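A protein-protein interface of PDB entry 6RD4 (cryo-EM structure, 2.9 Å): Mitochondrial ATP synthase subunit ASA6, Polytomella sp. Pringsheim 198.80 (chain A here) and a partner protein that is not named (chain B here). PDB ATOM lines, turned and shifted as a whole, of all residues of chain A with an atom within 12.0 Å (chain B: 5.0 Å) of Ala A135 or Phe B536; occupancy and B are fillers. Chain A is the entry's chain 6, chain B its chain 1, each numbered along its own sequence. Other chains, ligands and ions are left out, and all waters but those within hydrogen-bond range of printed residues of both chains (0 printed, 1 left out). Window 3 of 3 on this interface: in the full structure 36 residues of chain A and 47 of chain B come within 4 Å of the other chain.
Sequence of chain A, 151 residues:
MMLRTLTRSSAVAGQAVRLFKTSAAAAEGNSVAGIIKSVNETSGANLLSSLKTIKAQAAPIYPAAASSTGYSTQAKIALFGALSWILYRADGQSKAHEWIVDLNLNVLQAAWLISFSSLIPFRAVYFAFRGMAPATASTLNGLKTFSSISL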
ATOM      1  N   PRO A  60      11.708 -13.113   6.614  1.00  0.00           N
ATOM      2  CA  PRO A  60      11.100 -13.905   7.677  1.00  0.00           C
ATOM      3  C   PRO A  60       9.958 -14.744   7.143  1.00  0.00           C
ATOM      4  O   PRO A  60       9.355 -14.441   6.117  1.00  0.00           O
ATOM      5  CB  PRO A  60      10.605 -12.849   8.653  1.00  0.00           C
ATOM      6  CG  PRO A  60      10.381 -11.699   7.837  1.00  0.00           C
ATOM      7  CD  PRO A  60      11.424 -11.685   6.804  1.00  0.00           C
ATOM      8  N   TYR A  62       6.374 -15.897   6.894  1.00  0.00           N
ATOM      9  CA  TYR A  62       4.994 -15.555   7.180  1.00  0.00           C
ATOM     10  C   TYR A  62       4.200 -16.742   6.700  1.00  0.00           C
ATOM     11  O   TYR A  62       4.060 -16.917   5.476  1.00  0.00           O
ATOM     12  CB  TYR A  62       4.575 -14.293   6.447  1.00  0.00           C
ATOM     13  CG  TYR A  62       5.413 -13.098   6.765  1.00  0.00           C
ATOM     14  CD1 TYR A  62       5.762 -12.801   8.053  1.00  0.00           C
ATOM     15  CD2 TYR A  62       5.853 -12.262   5.767  1.00  0.00           C
ATOM     16  CE1 TYR A  62       6.518 -11.714   8.337  1.00  0.00           C
ATOM     17  CE2 TYR A  62       6.611 -11.176   6.051  1.00  0.00           C
ATOM     18  CZ  TYR A  62       6.935 -10.909   7.340  1.00  0.00           C
ATOM     19  OH  TYR A  62       7.692  -9.817   7.624  1.00  0.00           O
ATOM     20  N   TYR A 126     -12.621   0.277  18.199  1.00  0.00           N
ATOM     21  CA  TYR A 126     -11.367  -0.448  18.040  1.00  0.00           C
ATOM     22  C   TYR A 126     -10.178   0.474  18.207  1.00  0.00           C
ATOM     23  O   TYR A 126      -9.188   0.114  18.839  1.00  0.00           O
ATOM     24  CB  TYR A 126     -11.316  -1.115  16.674  1.00  0.00           C
ATOM     25  CG  TYR A 126     -10.015  -1.796  16.388  1.00  0.00           C
ATOM     26  CD1 TYR A 126      -9.729  -3.020  16.938  1.00  0.00           C
ATOM     27  CD2 TYR A 126      -9.071  -1.221  15.565  1.00  0.00           C
ATOM     28  CE1 TYR A 126      -8.549  -3.635  16.695  1.00  0.00           C
ATOM     29  CE2 TYR A 126      -7.890  -1.828  15.327  1.00  0.00           C
ATOM     30  CZ  TYR A 126      -7.639  -3.035  15.892  1.00  0.00           C
ATOM     31  OH  TYR A 126      -6.456  -3.654  15.649  1.00  0.00           O
ATOM     32  N   PHE A 127     -10.249   1.664  17.646  1.00  0.00           N
ATOM     33  CA  PHE A 127      -9.147   2.596  17.769  1.00  0.00           C
ATOM     34  C   PHE A 127      -9.175   3.351  19.074  1.00  0.00           C
ATOM     35  O   PHE A 127      -8.199   4.026  19.395  1.00  0.00           O
ATOM     36  CB  PHE A 127      -9.159   3.576  16.607  1.00  0.00           C
ATOM     37  CG  PHE A 127      -8.550   3.033  15.370  1.00  0.00           C
ATOM     38  CD1 PHE A 127      -7.193   3.015  15.217  1.00  0.00           C
ATOM     39  CD2 PHE A 127      -9.333   2.525  14.368  1.00  0.00           C
ATOM     40  CE1 PHE A 127      -6.637   2.499  14.089  1.00  0.00           C
ATOM     41  CE2 PHE A 127      -8.777   2.015  13.246  1.00  0.00           C
ATOM     42  CZ  PHE A 127      -7.433   2.003  13.107  1.00  0.00           C
ATOM     43  N   ALA A 128     -10.258   3.266  19.827  1.00  0.00           N
ATOM     44  CA  ALA A 128     -10.288   3.817  21.168  1.00  0.00           C
ATOM     45  C   ALA A 128      -9.714   2.867  22.187  1.00  0.00           C
ATOM     46  O   ALA A 128      -9.238   3.317  23.223  1.00  0.00           O
ATOM     47  CB  ALA A 128     -11.710   4.164  21.580  1.00  0.00           C
ATOM     48  N   PHE A 129      -9.780   1.567  21.942  1.00  0.00           N
ATOM     49  CA  PHE A 129      -9.112   0.632  22.833  1.00  0.00           C
ATOM     50  C   PHE A 129      -7.633   0.581  22.540  1.00  0.00           C
ATOM     51  O   PHE A 129      -6.842   0.288  23.429  1.00  0.00           O
ATOM     52  CB  PHE A 129      -9.708  -0.763  22.718  1.00  0.00           C
ATOM     53  CG  PHE A 129     -11.072  -0.900  23.330  1.00  0.00           C
ATOM     54  CD1 PHE A 129     -11.620   0.092  24.100  1.00  0.00           C
ATOM     55  CD2 PHE A 129     -11.804  -2.031  23.127  1.00  0.00           C
ATOM     56  CE1 PHE A 129     -12.852  -0.046  24.636  1.00  0.00           C
ATOM     57  CE2 PHE A 129     -13.032  -2.170  23.676  1.00  0.00           C
ATOM     58  CZ  PHE A 129     -13.553  -1.178  24.425  1.00  0.00           C
ATOM     59  N   ARG A 130      -7.238   0.886  21.309  1.00  0.00           N
ATOM     60  CA  ARG A 130      -5.827   0.981  20.967  1.00  0.00           C
ATOM     61  C   ARG A 130      -5.145   2.143  21.647  1.00  0.00           C
ATOM     62  O   ARG A 130      -3.927   2.123  21.779  1.00  0.00           O
ATOM     63  CB  ARG A 130      -5.655   1.125  19.471  1.00  0.00           C
ATOM     64  CG  ARG A 130      -5.667  -0.156  18.760  1.00  0.00           C
ATOM     65  CD  ARG A 130      -5.342   0.029  17.324  1.00  0.00           C
ATOM     66  NE  ARG A 130      -3.929   0.248  17.113  1.00  0.00           N
ATOM     67  CZ  ARG A 130      -3.075  -0.712  16.816  1.00  0.00           C
ATOM     68  NH1 ARG A 130      -3.486  -1.948  16.711  1.00  0.00           N
ATOM     69  NH2 ARG A 130      -1.805  -0.435  16.639  1.00  0.00           N
ATOM     70  N   GLY A 131      -5.880   3.160  22.044  1.00  0.00           N
ATOM     71  CA  GLY A 131      -5.320   4.242  22.813  1.00  0.00           C
ATOM     72  C   GLY A 131      -5.309   4.029  24.296  1.00  0.00           C
ATOM     73  O   GLY A 131      -4.682   4.802  25.009  1.00  0.00           O
ATOM     74  N   MET A 132      -5.998   3.005  24.791  1.00  0.00           N
ATOM     75  CA  MET A 132      -5.933   2.684  26.208  1.00  0.00           C
ATOM     76  C   MET A 132      -4.587   2.099  26.572  1.00  0.00           C
ATOM     77  O   MET A 132      -4.100   2.288  27.688  1.00  0.00           O
ATOM     78  CB  MET A 132      -7.017   1.688  26.591  1.00  0.00           C
ATOM     79  CG  MET A 132      -8.395   2.061  26.254  1.00  0.00           C
ATOM     80  SD  MET A 132      -9.514   0.815  26.842  1.00  0.00           S
ATOM     81  CE  MET A 132      -9.350   1.076  28.583  1.00  0.00           C
ATOM     82  N   ALA A 133      -4.028   1.379  25.707  1.00  0.00           N
ATOM     83  CA  ALA A 133      -2.746   0.743  25.880  1.00  0.00           C
ATOM     84  C   ALA A 133      -1.658   1.652  25.369  1.00  0.00           C
ATOM     85  O   ALA A 133      -1.714   2.063  24.216  1.00  0.00           O
ATOM     86  CB  ALA A 133      -2.700  -0.553  25.117  1.00  0.00           C
ATOM     87  N   PRO A 134      -0.644   1.972  26.168  1.00  0.00           N
ATOM     88  CA  PRO A 134       0.469   2.765  25.652  1.00  0.00           C
ATOM     89  C   PRO A 134       1.310   2.051  24.620  1.00  0.00           C
ATOM     90  O   PRO A 134       2.061   2.718  23.913  1.00  0.00           O
ATOM     91  CB  PRO A 134       1.286   3.062  26.906  1.00  0.00           C
ATOM     92  CG  PRO A 134       0.391   2.868  27.983  1.00  0.00           C
ATOM     93  CD  PRO A 134      -0.516   1.778  27.609  1.00  0.00           C
ATOM     94  N   ALA A 135       1.204   0.729  24.508  1.00  0.00           N
ATOM     95  CA  ALA A 135       1.940  -0.017  23.503  1.00  0.00           C
ATOM     96  C   ALA A 135       1.405   0.216  22.108  1.00  0.00           C
ATOM     97  O   ALA A 135       2.139   0.057  21.133  1.00  0.00           O
ATOM     98  CB  ALA A 135       1.882  -1.496  23.820  1.00  0.00           C
ATOM     99  N   THR A 136       0.137   0.552  21.976  1.00  0.00           N
ATOM    100  CA  THR A 136      -0.468   0.771  20.678  1.00  0.00           C
ATOM    101  C   THR A 136      -0.876   2.213  20.470  1.00  0.00           C
ATOM    102  O   THR A 136      -1.297   2.574  19.377  1.00  0.00           O
ATOM    103  CB  THR A 136      -1.685  -0.122  20.513  1.00  0.00           C
ATOM    104  OG1 THR A 136      -2.595   0.166  21.561  1.00  0.00           O
ATOM    105  CG2 THR A 136      -1.322  -1.542  20.624  1.00  0.00           C
ATOM    106  N   ALA A 137      -0.773   3.042  21.492  1.00  0.00           N
ATOM    107  CA  ALA A 137      -1.080   4.449  21.376  1.00  0.00           C
ATOM    108  C   ALA A 137       0.002   5.237  20.662  1.00  0.00           C
ATOM    109  O   ALA A 137      -0.229   6.398  20.321  1.00  0.00           O
ATOM    110  CB  ALA A 137      -1.308   5.036  22.762  1.00  0.00           C
ATOM    111  N   SER A 138       1.169   4.648  20.424  1.00  0.00           N
ATOM    112  CA  SER A 138       2.276   5.325  19.775  1.00  0.00           C
ATOM    113  C   SER A 138       2.933   4.338  18.833  1.00  0.00           C
ATOM    114  O   SER A 138       2.432   3.239  18.605  1.00  0.00           O
ATOM    115  CB  SER A 138       3.272   5.845  20.809  1.00  0.00           C
ATOM    116  OG  SER A 138       2.667   6.769  21.675  1.00  0.00           O
ATOM    117  N   THR A 139       4.072   4.731  18.282  1.00  0.00           N
ATOM    118  CA  THR A 139       4.921   3.866  17.488  1.00  0.00           C
ATOM    119  C   THR A 139       6.125   3.518  18.348  1.00  0.00           C
ATOM    120  O   THR A 139       6.432   4.238  19.296  1.00  0.00           O
ATOM    121  CB  THR A 139       5.352   4.593  16.216  1.00  0.00           C
ATOM    122  OG1 THR A 139       4.226   5.284  15.683  1.00  0.00           O
ATOM    123  CG2 THR A 139       5.815   3.621  15.142  1.00  0.00           C
ATOM    124  N   LEU A 140       6.795   2.409  18.042  1.00  0.00           N
ATOM    125  CA  LEU A 140       8.047   2.108  18.712  1.00  0.00           C
ATOM    126  C   LEU A 140       9.101   3.158  18.423  1.00  0.00           C
ATOM    127  O   LEU A 140       9.105   3.791  17.372  1.00  0.00           O
ATOM    128  CB  LEU A 140       8.586   0.760  18.298  1.00  0.00           C
ATOM    129  CG  LEU A 140       8.168  -0.395  19.149  1.00  0.00           C
ATOM    130  CD1 LEU A 140       8.864  -1.510  18.580  1.00  0.00           C
ATOM    131  CD2 LEU A 140       8.675  -0.165  20.508  1.00  0.00           C
ATOM    132  N   ASN A 141      10.022   3.320  19.357  1.00  0.00           N
ATOM    133  CA  ASN A 141      10.798   4.531  19.389  1.00  0.00           C
ATOM    134  C   ASN A 141      12.305   4.367  19.367  1.00  0.00           C
ATOM    135  O   ASN A 141      12.992   5.362  19.143  1.00  0.00           O
ATOM    136  CB  ASN A 141      10.438   5.351  20.619  1.00  0.00           C
ATOM    137  CG  ASN A 141      10.598   6.813  20.390  1.00  0.00           C
ATOM    138  OD1 ASN A 141      10.540   7.273  19.256  1.00  0.00           O
ATOM    139  ND2 ASN A 141      10.821   7.562  21.460  1.00  0.00           N
ATOM    140  N   GLY A 142      12.859   3.196  19.584  1.00  0.00           N
ATOM    141  CA  GLY A 142      14.303   3.106  19.623  1.00  0.00           C
ATOM    142  C   GLY A 142      14.944   3.086  18.260  1.00  0.00           C
ATOM    143  O   GLY A 142      14.286   3.259  17.242  1.00  0.00           O
ATOM    144  N   HIS B 531      12.022  -5.382  12.258  1.00  0.00           N
ATOM    145  CA  HIS B 531      10.942  -6.336  12.161  1.00  0.00           C
ATOM    146  C   HIS B 531       9.970  -6.216  13.307  1.00  0.00           C
ATOM    147  O   HIS B 531       8.784  -6.463  13.120  1.00  0.00           O
ATOM    148  CB  HIS B 531      11.490  -7.742  12.114  1.00  0.00           C
ATOM    149  CG  HIS B 531      10.460  -8.767  11.804  1.00  0.00           C
ATOM    150  ND1 HIS B 531      10.062  -9.710  12.713  1.00  0.00           N
ATOM    151  CD2 HIS B 531       9.718  -8.972  10.699  1.00  0.00           C
ATOM    152  CE1 HIS B 531       9.137 -10.473  12.172  1.00  0.00           C
ATOM    153  NE2 HIS B 531       8.911 -10.048  10.948  1.00  0.00           N
ATOM    154  N   ILE B 532      10.439  -5.848  14.492  1.00  0.00           N
ATOM    155  CA  ILE B 532       9.526  -5.538  15.576  1.00  0.00           C
ATOM    156  C   ILE B 532       8.714  -4.310  15.232  1.00  0.00           C
ATOM    157  O   ILE B 532       7.491  -4.349  15.275  1.00  0.00           O
ATOM    158  CB  ILE B 532      10.288  -5.359  16.892  1.00  0.00           C
ATOM    159  CG1 ILE B 532      10.962  -6.650  17.272  1.00  0.00           C
ATOM    160  CG2 ILE B 532       9.362  -5.051  17.959  1.00  0.00           C
ATOM    161  CD1 ILE B 532      11.840  -6.543  18.455  1.00  0.00           C
ATOM    162  N   GLN B 533       9.375  -3.236  14.804  1.00  0.00           N
ATOM    163  CA  GLN B 533       8.697  -1.971  14.544  1.00  0.00           C
ATOM    164  C   GLN B 533       7.682  -2.062  13.423  1.00  0.00           C
ATOM    165  O   GLN B 533       6.634  -1.419  13.480  1.00  0.00           O
ATOM    166  CB  GLN B 533       9.718  -0.906  14.214  1.00  0.00           C
ATOM    167  CG  GLN B 533       9.141   0.448  14.165  1.00  0.00           C
ATOM    168  CD  GLN B 533      10.136   1.449  13.786  1.00  0.00           C
ATOM    169  OE1 GLN B 533      10.809   1.314  12.773  1.00  0.00           O
ATOM    170  NE2 GLN B 533      10.266   2.475  14.600  1.00  0.00           N
ATOM    171  N   LYS B 534       7.942  -2.897  12.433  1.00  0.00           N
ATOM    172  CA  LYS B 534       7.026  -3.067  11.322  1.00  0.00           C
ATOM    173  C   LYS B 534       5.768  -3.796  11.746  1.00  0.00           C
ATOM    174  O   LYS B 534       4.706  -3.586  11.165  1.00  0.00           O
ATOM    175  CB  LYS B 534       7.748  -3.831  10.227  1.00  0.00           C
ATOM    176  CG  LYS B 534       7.063  -3.947   8.924  1.00  0.00           C
ATOM    177  CD  LYS B 534       7.783  -4.928   8.073  1.00  0.00           C
ATOM    178  CE  LYS B 534       6.957  -5.278   6.884  1.00  0.00           C
ATOM    179  NZ  LYS B 534       7.601  -6.364   6.091  1.00  0.00           N
ATOM    180  N   HIS B 535       5.862  -4.634  12.766  1.00  0.00           N
ATOM    181  CA  HIS B 535       4.819  -5.574  13.114  1.00  0.00           C
ATOM    182  C   HIS B 535       4.286  -5.442  14.524  1.00  0.00           C
ATOM    183  O   HIS B 535       3.298  -6.099  14.827  1.00  0.00           O
ATOM    184  CB  HIS B 535       5.327  -7.007  12.940  1.00  0.00           C
ATOM    185  CG  HIS B 535       5.436  -7.447  11.519  1.00  0.00           C
ATOM    186  ND1 HIS B 535       4.338  -7.678  10.730  1.00  0.00           N
ATOM    187  CD2 HIS B 535       6.511  -7.722  10.753  1.00  0.00           C
ATOM    188  CE1 HIS B 535       4.731  -8.054   9.531  1.00  0.00           C
ATOM    189  NE2 HIS B 535       6.045  -8.090   9.521  1.00  0.00           N
ATOM    190  N   PHE B 536       4.905  -4.661  15.399  1.00  0.00           N
ATOM    191  CA  PHE B 536       4.454  -4.583  16.779  1.00  0.00           C
ATOM    192  C   PHE B 536       3.151  -3.826  16.860  1.00  0.00           C
ATOM    193  O   PHE B 536       3.026  -2.737  16.302  1.00  0.00           O
ATOM    194  CB  PHE B 536       5.484  -3.880  17.643  1.00  0.00           C
ATOM    195  CG  PHE B 536       5.215  -3.971  19.085  1.00  0.00           C
ATOM    196  CD1 PHE B 536       5.454  -5.127  19.763  1.00  0.00           C
ATOM    197  CD2 PHE B 536       4.727  -2.896  19.767  1.00  0.00           C
ATOM    198  CE1 PHE B 536       5.199  -5.205  21.072  1.00  0.00           C
ATOM    199  CE2 PHE B 536       4.477  -2.984  21.065  1.00  0.00           C
ATOM    200  CZ  PHE B 536       4.713  -4.135  21.722  1.00  0.00           C
ATOM    201  N   GLY B 537       2.186  -4.390  17.570  1.00  0.00           N
ATOM    202  CA  GLY B 537       0.901  -3.768  17.697  1.00  0.00           C
ATOM    203  C   GLY B 537       0.016  -3.939  16.498  1.00  0.00           C
ATOM    204  O   GLY B 537      -1.057  -3.339  16.451  1.00  0.00           O
ATOM    205  N   ILE B 538       0.436  -4.723  15.519  1.00  0.00           N
ATOM    206  CA  ILE B 538      -0.383  -5.018  14.359  1.00  0.00           C
ATOM    207  C   ILE B 538      -0.564  -6.519  14.284  1.00  0.00           C
ATOM    208  O   ILE B 538      -1.664  -7.018  14.503  1.00  0.00           O
ATOM    209  CB  ILE B 538       0.242  -4.462  13.072  1.00  0.00           C
ATOM    210  CG1 ILE B 538       0.254  -2.952  13.097  1.00  0.00           C
ATOM    211  CG2 ILE B 538      -0.539  -4.875  11.903  1.00  0.00           C
ATOM    212  CD1 ILE B 538       1.250  -2.370  12.212  1.00  0.00           C
ATOM    213  N   LEU B 540       2.395  -8.960  15.205  1.00  0.00           N
ATOM    214  CA  LEU B 540       3.559  -9.727  15.617  1.00  0.00           C
ATOM    215  C   LEU B 540       3.153 -10.700  16.703  1.00  0.00           C
ATOM    216  O   LEU B 540       2.506 -10.294  17.655  1.00  0.00           O
ATOM    217  CB  LEU B 540       4.639  -8.802  16.138  1.00  0.00           C
ATOM    218  CG  LEU B 540       6.062  -9.205  16.496  1.00  0.00           C
ATOM    219  CD1 LEU B 540       6.772  -9.753  15.355  1.00  0.00           C
ATOM    220  CD2 LEU B 540       6.731  -8.001  16.937  1.00  0.00           C
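The side-chain amide nitrogen (NE2) of Gln B533 is in hydrogen-bond range of the backbone carbonyl oxygen (O) of Leu A140 (3.3 Å). NE2 of His B535 lies within hydrogen-bond range of OH of Tyr A62. NH1 of Arg A130 sits at hydrogen-bond distance from O of Gly B537, 2.8 Å away.
The backbone carbonyl oxygen (O) of His B535 sits at hydrogen-bond distance from the backbone NH (N) of Leu B540, at 3.0 Å. The backbone NH (N) of Ala A137 sits at hydrogen-bond distance from the backbone carbonyl oxygen (O) of Arg A130, 3.3 Å away.
Among the printed residues, merely in contact across the chains: Tyr A62 with His B531 (3.5 Å), Leu A140 with Ile B532 (3.6 Å), Tyr A62 with Lys B534 (3.8 Å), Pro A60 with His B531 (3.8 Å) and Ala A135 with Phe B536 (3.8 Å).
Ala A135 touches just one residue of chain B: Phe B536. Of chain A, only Ala A135 (3.8 Å) comes within 4 Å of Phe B536. His B535 touches one residue of chain A. Gly B537 touches one residue of chain A. No residue of chain A comes within 4 Å of Leu B540. Of the printed residues of chain A, Gln B533 touches Leu A140. Of the printed residues of chain A, Lys B534 touches Tyr A62 (3.8 Å). Phe A127 touches none of the printed residues of chain B. Ala A137 touches none of the printed residues of chain B. The nearest printed residue of chain B that does not touch Ala A135 is Gly B537 (5.3 Å).
Of the 19 printed residues of chain A, 5 touch a printed residue of chain B. Of the 9 printed residues of chain B, 7 touch a printed residue of chain A. Printed residues of chain B that touch a printed residue of chain A: His B531, Ile B532, Gln B533, Lys B534, His B535, Phe B536 and Gly B537. Along chain B the printed residues that touch a printed residue of chain A span positions 531 to 537. Among the printed residues, 8 pairs touch across the chains. Among the printed residues, no Asp or Glu carboxylate lies within 4 Å of a Lys or Arg side-chain nitrogen of the other chain.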
